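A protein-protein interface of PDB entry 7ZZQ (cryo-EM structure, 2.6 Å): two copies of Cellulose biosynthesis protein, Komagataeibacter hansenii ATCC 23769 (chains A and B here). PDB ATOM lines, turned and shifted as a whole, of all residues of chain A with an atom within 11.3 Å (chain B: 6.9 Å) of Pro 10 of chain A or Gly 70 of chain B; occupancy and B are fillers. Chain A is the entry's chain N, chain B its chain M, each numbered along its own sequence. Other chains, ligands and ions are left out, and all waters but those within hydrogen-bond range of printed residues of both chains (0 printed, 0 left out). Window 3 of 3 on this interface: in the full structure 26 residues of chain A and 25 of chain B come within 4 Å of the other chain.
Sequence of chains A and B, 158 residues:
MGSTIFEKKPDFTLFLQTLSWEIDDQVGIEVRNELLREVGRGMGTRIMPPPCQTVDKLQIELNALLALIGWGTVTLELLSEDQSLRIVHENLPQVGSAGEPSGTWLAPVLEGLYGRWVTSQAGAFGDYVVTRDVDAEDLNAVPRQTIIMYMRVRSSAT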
ATOM      1  N   LYS A   9      10.796  15.720 -34.819  1.00  0.00           N
ATOM      2  CA  LYS A   9      10.934  15.937 -33.383  1.00  0.00           C
ATOM      3  C   LYS A   9       9.877  15.161 -32.605  1.00  0.00           C
ATOM      4  O   LYS A   9       8.683  15.296 -32.871  1.00  0.00           O
ATOM      5  CB  LYS A   9      10.838  17.426 -33.052  1.00  0.00           C
ATOM      6  CG  LYS A   9      11.977  17.943 -32.193  1.00  0.00           C
ATOM      7  CD  LYS A   9      11.732  19.376 -31.760  1.00  0.00           C
ATOM      8  CE  LYS A   9      12.412  19.671 -30.433  1.00  0.00           C
ATOM      9  NZ  LYS A   9      13.814  19.170 -30.404  1.00  0.00           N
ATOM     10  N   PRO A  10      10.318  14.341 -31.652  1.00  0.00           N
ATOM     11  CA  PRO A  10       9.362  13.588 -30.832  1.00  0.00           C
ATOM     12  C   PRO A  10       8.475  14.516 -30.018  1.00  0.00           C
ATOM     13  O   PRO A  10       8.905  15.573 -29.554  1.00  0.00           O
ATOM     14  CB  PRO A  10      10.260  12.732 -29.929  1.00  0.00           C
ATOM     15  CG  PRO A  10      11.598  12.727 -30.590  1.00  0.00           C
ATOM     16  CD  PRO A  10      11.715  14.027 -31.313  1.00  0.00           C
ATOM     17  N   ASP A  11       7.223  14.105 -29.846  1.00  0.00           N
ATOM     18  CA  ASP A  11       6.252  14.837 -29.045  1.00  0.00           C
ATOM     19  C   ASP A  11       5.987  14.050 -27.770  1.00  0.00           C
ATOM     20  O   ASP A  11       5.577  12.887 -27.829  1.00  0.00           O
ATOM     21  CB  ASP A  11       4.957  15.062 -29.824  1.00  0.00           C
ATOM     22  CG  ASP A  11       3.818  15.524 -28.939  1.00  0.00           C
ATOM     23  OD1 ASP A  11       3.839  16.693 -28.500  1.00  0.00           O
ATOM     24  OD2 ASP A  11       2.899  14.718 -28.683  1.00  0.00           O
ATOM     25  N   PHE A  12       6.225  14.682 -26.624  1.00  0.00           N
ATOM     26  CA  PHE A  12       6.051  14.043 -25.328  1.00  0.00           C
ATOM     27  C   PHE A  12       4.797  14.512 -24.605  1.00  0.00           C
ATOM     28  O   PHE A  12       4.628  14.204 -23.423  1.00  0.00           O
ATOM     29  CB  PHE A  12       7.279  14.290 -24.452  1.00  0.00           C
ATOM     30  CG  PHE A  12       8.549  13.737 -25.023  1.00  0.00           C
ATOM     31  CD1 PHE A  12       8.716  12.372 -25.184  1.00  0.00           C
ATOM     32  CD2 PHE A  12       9.577  14.582 -25.403  1.00  0.00           C
ATOM     33  CE1 PHE A  12       9.885  11.863 -25.709  1.00  0.00           C
ATOM     34  CE2 PHE A  12      10.747  14.077 -25.929  1.00  0.00           C
ATOM     35  CZ  PHE A  12      10.901  12.716 -26.082  1.00  0.00           C
ATOM     36  N   THR A  13       3.918  15.250 -25.286  1.00  0.00           N
ATOM     37  CA  THR A  13       2.727  15.779 -24.628  1.00  0.00           C
ATOM     38  C   THR A  13       1.821  14.655 -24.140  1.00  0.00           C
ATOM     39  O   THR A  13       1.442  14.618 -22.965  1.00  0.00           O
ATOM     40  CB  THR A  13       1.969  16.703 -25.581  1.00  0.00           C
ATOM     41  OG1 THR A  13       2.902  17.501 -26.319  1.00  0.00           O
ATOM     42  CG2 THR A  13       1.039  17.617 -24.802  1.00  0.00           C
ATOM     43  N   LEU A  14       1.471  13.723 -25.027  1.00  0.00           N
ATOM     44  CA  LEU A  14       0.619  12.606 -24.632  1.00  0.00           C
ATOM     45  C   LEU A  14       1.315  11.711 -23.615  1.00  0.00           C
ATOM     46  O   LEU A  14       0.686  11.239 -22.657  1.00  0.00           O
ATOM     47  CB  LEU A  14       0.209  11.801 -25.864  1.00  0.00           C
ATOM     48  CG  LEU A  14      -0.921  10.795 -25.653  1.00  0.00           C
ATOM     49  CD1 LEU A  14      -2.272  11.461 -25.852  1.00  0.00           C
ATOM     50  CD2 LEU A  14      -0.758   9.612 -26.589  1.00  0.00           C
ATOM     51  N   PHE A  15       2.612  11.463 -23.811  1.00  0.00           N
ATOM     52  CA  PHE A  15       3.365  10.670 -22.849  1.00  0.00           C
ATOM     53  C   PHE A  15       3.378  11.335 -21.481  1.00  0.00           C
ATOM     54  O   PHE A  15       3.215  10.665 -20.458  1.00  0.00           O
ATOM     55  CB  PHE A  15       4.793  10.446 -23.343  1.00  0.00           C
ATOM     56  CG  PHE A  15       5.731   9.974 -22.272  1.00  0.00           C
ATOM     57  CD1 PHE A  15       5.685   8.667 -21.821  1.00  0.00           C
ATOM     58  CD2 PHE A  15       6.650  10.840 -21.705  1.00  0.00           C
ATOM     59  CE1 PHE A  15       6.539   8.232 -20.829  1.00  0.00           C
ATOM     60  CE2 PHE A  15       7.507  10.409 -20.714  1.00  0.00           C
ATOM     61  CZ  PHE A  15       7.451   9.104 -20.275  1.00  0.00           C
ATOM     62  N   LEU A  16       3.569  12.655 -21.441  1.00  0.00           N
ATOM     63  CA  LEU A  16       3.586  13.355 -20.161  1.00  0.00           C
ATOM     64  C   LEU A  16       2.206  13.371 -19.517  1.00  0.00           C
ATOM     65  O   LEU A  16       2.091  13.276 -18.291  1.00  0.00           O
ATOM     66  CB  LEU A  16       4.118  14.774 -20.343  1.00  0.00           C
ATOM     67  CG  LEU A  16       5.640  14.922 -20.339  1.00  0.00           C
ATOM     68  CD1 LEU A  16       6.033  16.347 -20.010  1.00  0.00           C
ATOM     69  CD2 LEU A  16       6.280  13.951 -19.357  1.00  0.00           C
ATOM     70  N   ILE A  69      14.139  26.640 -23.666  1.00  0.00           N
ATOM     71  CA  ILE A  69      13.327  25.430 -23.606  1.00  0.00           C
ATOM     72  C   ILE A  69      11.852  25.707 -23.835  1.00  0.00           C
ATOM     73  O   ILE A  69      11.057  24.757 -23.892  1.00  0.00           O
ATOM     74  CB  ILE A  69      13.528  24.685 -22.274  1.00  0.00           C
ATOM     75  CG1 ILE A  69      13.258  25.618 -21.093  1.00  0.00           C
ATOM     76  CG2 ILE A  69      14.932  24.111 -22.194  1.00  0.00           C
ATOM     77  CD1 ILE A  69      13.238  24.917 -19.757  1.00  0.00           C
ATOM     78  N   LYS B   9       5.718  25.869 -28.738  1.00  0.00           N
ATOM     79  CA  LYS B   9       5.611  24.506 -28.231  1.00  0.00           C
ATOM     80  C   LYS B   9       6.738  24.208 -27.248  1.00  0.00           C
ATOM     81  O   LYS B   9       7.912  24.237 -27.619  1.00  0.00           O
ATOM     82  CB  LYS B   9       5.629  23.501 -29.382  1.00  0.00           C
ATOM     83  CG  LYS B   9       5.612  22.046 -28.944  1.00  0.00           C
ATOM     84  CD  LYS B   9       5.492  21.115 -30.139  1.00  0.00           C
ATOM     85  CE  LYS B   9       5.447  19.658 -29.707  1.00  0.00           C
ATOM     86  NZ  LYS B   9       6.609  18.886 -30.225  1.00  0.00           N
ATOM     87  N   ASP B  11       9.474  22.411 -24.937  1.00  0.00           N
ATOM     88  CA  ASP B  11      10.365  21.276 -25.128  1.00  0.00           C
ATOM     89  C   ASP B  11      10.546  20.570 -23.790  1.00  0.00           C
ATOM     90  O   ASP B  11      10.933  21.199 -22.800  1.00  0.00           O
ATOM     91  CB  ASP B  11      11.708  21.732 -25.699  1.00  0.00           C
ATOM     92  CG  ASP B  11      12.810  20.702 -25.516  1.00  0.00           C
ATOM     93  OD1 ASP B  11      13.384  20.617 -24.409  1.00  0.00           O
ATOM     94  OD2 ASP B  11      13.104  19.977 -26.488  1.00  0.00           O
ATOM     95  N   THR B  13      12.514  17.750 -23.457  1.00  0.00           N
ATOM     96  CA  THR B  13      13.667  16.859 -23.540  1.00  0.00           C
ATOM     97  C   THR B  13      14.539  16.959 -22.294  1.00  0.00           C
ATOM     98  O   THR B  13      14.881  15.941 -21.684  1.00  0.00           O
ATOM     99  CB  THR B  13      14.484  17.174 -24.792  1.00  0.00           C
ATOM    100  OG1 THR B  13      13.605  17.309 -25.916  1.00  0.00           O
ATOM    101  CG2 THR B  13      15.483  16.062 -25.067  1.00  0.00           C
ATOM    102  N   ALA B  64       1.113   4.901 -38.620  1.00  0.00           N
ATOM    103  CA  ALA B  64       0.362   6.153 -38.611  1.00  0.00           C
ATOM    104  C   ALA B  64       0.225   6.703 -37.195  1.00  0.00           C
ATOM    105  O   ALA B  64       0.395   7.908 -36.964  1.00  0.00           O
ATOM    106  CB  ALA B  64      -1.012   5.947 -39.246  1.00  0.00           C
ATOM    107  N   LEU B  65      -0.068   5.828 -36.231  1.00  0.00           N
ATOM    108  CA  LEU B  65      -0.168   6.265 -34.840  1.00  0.00           C
ATOM    109  C   LEU B  65       1.162   6.809 -34.332  1.00  0.00           C
ATOM    110  O   LEU B  65       1.197   7.811 -33.610  1.00  0.00           O
ATOM    111  CB  LEU B  65      -0.640   5.110 -33.959  1.00  0.00           C
ATOM    112  CG  LEU B  65      -2.118   4.740 -34.044  1.00  0.00           C
ATOM    113  CD1 LEU B  65      -2.369   3.444 -33.305  1.00  0.00           C
ATOM    114  CD2 LEU B  65      -2.979   5.860 -33.487  1.00  0.00           C
ATOM    115  N   LEU B  66       2.267   6.148 -34.683  1.00  0.00           N
ATOM    116  CA  LEU B  66       3.581   6.615 -34.252  1.00  0.00           C
ATOM    117  C   LEU B  66       3.937   7.948 -34.896  1.00  0.00           C
ATOM    118  O   LEU B  66       4.526   8.818 -34.246  1.00  0.00           O
ATOM    119  CB  LEU B  66       4.644   5.564 -34.570  1.00  0.00           C
ATOM    120  CG  LEU B  66       4.596   4.283 -33.739  1.00  0.00           C
ATOM    121  CD1 LEU B  66       5.435   3.198 -34.389  1.00  0.00           C
ATOM    122  CD2 LEU B  66       5.058   4.549 -32.315  1.00  0.00           C
ATOM    123  N   ALA B  67       3.596   8.123 -36.176  1.00  0.00           N
ATOM    124  CA  ALA B  67       3.831   9.393 -36.849  1.00  0.00           C
ATOM    125  C   ALA B  67       2.944  10.502 -36.304  1.00  0.00           C
ATOM    126  O   ALA B  67       3.287  11.680 -36.449  1.00  0.00           O
ATOM    127  CB  ALA B  67       3.609   9.242 -38.355  1.00  0.00           C
ATOM    128  N   LEU B  68       1.810  10.150 -35.696  1.00  0.00           N
ATOM    129  CA  LEU B  68       0.988  11.159 -35.038  1.00  0.00           C
ATOM    130  C   LEU B  68       1.757  11.851 -33.917  1.00  0.00           C
ATOM    131  O   LEU B  68       1.669  13.073 -33.757  1.00  0.00           O
ATOM    132  CB  LEU B  68      -0.291  10.524 -34.495  1.00  0.00           C
ATOM    133  CG  LEU B  68      -1.372  11.487 -34.003  1.00  0.00           C
ATOM    134  CD1 LEU B  68      -1.930  12.302 -35.157  1.00  0.00           C
ATOM    135  CD2 LEU B  68      -2.479  10.732 -33.287  1.00  0.00           C
ATOM    136  N   ILE B  69       2.518  11.087 -33.134  1.00  0.00           N
ATOM    137  CA  ILE B  69       3.294  11.628 -32.025  1.00  0.00           C
ATOM    138  C   ILE B  69       4.778  11.701 -32.332  1.00  0.00           C
ATOM    139  O   ILE B  69       5.546  12.207 -31.501  1.00  0.00           O
ATOM    140  CB  ILE B  69       3.059  10.825 -30.732  1.00  0.00           C
ATOM    141  CG1 ILE B  69       3.296   9.335 -30.977  1.00  0.00           C
ATOM    142  CG2 ILE B  69       1.655  11.065 -30.205  1.00  0.00           C
ATOM    143  CD1 ILE B  69       3.340   8.508 -29.714  1.00  0.00           C
ATOM    144  N   GLY B  70       5.211  11.218 -33.492  1.00  0.00           N
ATOM    145  CA  GLY B  70       6.615  11.278 -33.865  1.00  0.00           C
ATOM    146  C   GLY B  70       7.542  10.456 -32.995  1.00  0.00           C
ATOM    147  O   GLY B  70       8.625  10.932 -32.631  1.00  0.00           O
ATOM    148  N   TRP B  71       7.151   9.229 -32.657  1.00  0.00           N
ATOM    149  CA  TRP B  71       7.949   8.364 -31.800  1.00  0.00           C
ATOM    150  C   TRP B  71       8.720   7.305 -32.577  1.00  0.00           C
ATOM    151  O   TRP B  71       9.310   6.410 -31.962  1.00  0.00           O
ATOM    152  CB  TRP B  71       7.059   7.697 -30.751  1.00  0.00           C
ATOM    153  CG  TRP B  71       6.963   8.466 -29.469  1.00  0.00           C
ATOM    154  CD1 TRP B  71       6.741   9.803 -29.332  1.00  0.00           C
ATOM    155  CD2 TRP B  71       7.082   7.942 -28.142  1.00  0.00           C
ATOM    156  NE1 TRP B  71       6.715  10.146 -28.004  1.00  0.00           N
ATOM    157  CE2 TRP B  71       6.921   9.020 -27.252  1.00  0.00           C
ATOM    158  CE3 TRP B  71       7.309   6.666 -27.620  1.00  0.00           C
ATOM    159  CZ2 TRP B  71       6.981   8.862 -25.869  1.00  0.00           C
ATOM    160  CZ3 TRP B  71       7.369   6.511 -26.248  1.00  0.00           C
ATOM    161  CH2 TRP B  71       7.204   7.602 -25.389  1.00  0.00           C
ATOM    162  N   GLY B  72       8.729   7.379 -33.905  1.00  0.00           N
ATOM    163  CA  GLY B  72       9.517   6.456 -34.698  1.00  0.00           C
ATOM    164  C   GLY B  72       8.708   5.650 -35.692  1.00  0.00           C
ATOM    165  O   GLY B  72       7.601   6.044 -36.068  1.00  0.00           O
ATOM    166  N   ASN B  91      14.022   4.374 -34.294  1.00  0.00           N
ATOM    167  CA  ASN B  91      13.992   5.776 -33.871  1.00  0.00           C
ATOM    168  C   ASN B  91      13.117   5.979 -32.637  1.00  0.00           C
ATOM    169  O   ASN B  91      12.223   6.828 -32.610  1.00  0.00           O
ATOM    170  CB  ASN B  91      13.548   6.686 -35.019  1.00  0.00           C
ATOM    171  CG  ASN B  91      14.472   6.607 -36.215  1.00  0.00           C
ATOM    172  OD1 ASN B  91      15.655   6.929 -36.122  1.00  0.00           O
ATOM    173  ND2 ASN B  91      13.936   6.173 -37.349  1.00  0.00           N
ATOM    174  N   LEU B  92      13.382   5.191 -31.605  1.00  0.00           N
ATOM    175  CA  LEU B  92      12.781   5.452 -30.305  1.00  0.00           C
ATOM    176  C   LEU B  92      13.312   6.778 -29.770  1.00  0.00           C
ATOM    177  O   LEU B  92      14.524   7.014 -29.818  1.00  0.00           O
ATOM    178  CB  LEU B  92      13.094   4.319 -29.330  1.00  0.00           C
ATOM    179  CG  LEU B  92      12.974   4.652 -27.841  1.00  0.00           C
ATOM    180  CD1 LEU B  92      11.536   4.533 -27.365  1.00  0.00           C
ATOM    181  CD2 LEU B  92      13.888   3.771 -27.008  1.00  0.00           C
ATOM    182  N   PRO B  93      12.449   7.670 -29.281  1.00  0.00           N
ATOM    183  CA  PRO B  93      12.937   8.959 -28.775  1.00  0.00           C
ATOM    184  C   PRO B  93      13.942   8.773 -27.648  1.00  0.00           C
ATOM    185  O   PRO B  93      13.749   7.959 -26.742  1.00  0.00           O
ATOM    186  CB  PRO B  93      11.661   9.652 -28.284  1.00  0.00           C
ATOM    187  CG  PRO B  93      10.560   9.003 -29.046  1.00  0.00           C
ATOM    188  CD  PRO B  93      10.980   7.580 -29.240  1.00  0.00           C
ATOM    189  N   GLN B  94      15.022   9.544 -27.712  1.00  0.00           N
ATOM    190  CA  GLN B  94      16.114   9.453 -26.753  1.00  0.00           C
ATOM    191  C   GLN B  94      16.047  10.623 -25.784  1.00  0.00           C
ATOM    192  O   GLN B  94      16.015  11.783 -26.204  1.00  0.00           O
ATOM    193  CB  GLN B  94      17.466   9.437 -27.470  1.00  0.00           C
ATOM    194  CG  GLN B  94      18.626   9.007 -26.592  1.00  0.00           C
ATOM    195  CD  GLN B  94      19.973   9.349 -27.195  1.00  0.00           C
ATOM    196  OE1 GLN B  94      20.508  10.433 -26.970  1.00  0.00           O
ATOM    197  NE2 GLN B  94      20.529   8.423 -27.966  1.00  0.00           N
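The backbone NH (N) of Asp 11 of chain B sits at hydrogen-bond distance from the backbone carbonyl oxygen (O) of Ile 69 of chain A, 3.0 Å away.
NE1 of Trp 71 of chain B is in hydrogen-bond range of O of Asp 11 of chain A, at 3.0 Å.
The side-chain amino group (NZ) of Lys 9 of chain B lies within salt-bridge range of the side-chain carboxylate (OD1) of Asp 11 of chain A, 3.9 Å away.
The backbone NH (N) of Asp 11 of chain A sits at hydrogen-bond distance from the backbone carbonyl oxygen (O) of Ile 69 of chain B (3.0 Å).
The side-chain carboxylate (OD2) of Asp 11 of chain B sits at hydrogen-bond distance from the side-chain hydroxyl (OG1) of Thr 13 of chain B.
The backbone carbonyl oxygen (O) of Leu 66 of chain B sits at hydrogen-bond distance from the backbone NH (N) of Trp 71 of chain B (3.1 Å).
OD1 of Asp 11 of chain A is in hydrogen-bond range of OG1 of Thr 13 of chain A, 2.5 Å away.
O of Gly 70 of chain B touches CA of Pro 10 of chain A (3.3 Å).
CB of Pro 93 of chain B touches CB of Pro 10 of chain A, 3.8 Å away.
Phe 12 of chain A touches Trp 71 of chain B (CD1 to CZ2, 3.97 Å).
Pro 93 of chain B touches Phe 12 of chain A.
Trp 71 of chain B touches Phe 15 of chain A.
Of the printed residues of chain B, Pro 10 of chain A touches Gly 70 and Pro 93.
Of the printed residues of chain B, Phe 15 of chain A touches Trp 71.
Printed residues of chain A within 4 Å of Asp 11 of chain B: Ile 69 (3.0 Å).
No residue of chain A comes within 4 Å of Ala 67 of chain B.
Leu 68 of chain B touches none of the printed residues of chain A.
Of the printed residues of chain A, Ile 69 of chain B touches Asp 11 (3.0 Å).
Gly 70 of chain B touches just one residue of chain A: Pro 10.
Of the printed residues of chain A, Trp 71 of chain B touches Asp 11 (3.0 Å), Phe 12 (3.97 Å) and Phe 15 (3.7 Å).
Of chain A, only Pro 10 and Phe 12 come within 4 Å of Pro 93 of chain B.
The nearest residue of chain A that does not touch Gly 70 of chain B is Lys 9 of chain A (4.4 Å).
Printed residues of chain A that touch a printed residue of chain B: Pro 10, Asp 11, Phe 12, Phe 15 and Ile 69.
Hydrophobic or aromatic side chains of chain A that line the printed part of chain B: Pro 10, Phe 12 and Phe 15.
Of the 16 printed residues of chain B, 6 touch a printed residue of chain A.
Hydrophobic or aromatic side chains of chain B within 4 Å of the printed part of chain A: Trp 71 and Pro 93.
Among the printed residues, 9 pairs touch across the chains.
Among the printed residues, Asp or Glu carboxylates within 4 Å of a Lys or Arg side-chain nitrogen of the other chain: Asp 11 of chain A with Lys 9 of chain B (3.9 Å).
Asp 11 of chain A touches Lys 9 of chain B, but with the chains exchanged Lys 9 of chain A does not touch Asp 11 of chain B (4.02 Å).
Asp 11 of chain A touches Ile 69 of chain B, and with the chains exchanged Ile 69 of chain A touches Asp 11 of chain B.
4 positions are printed for both chains.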
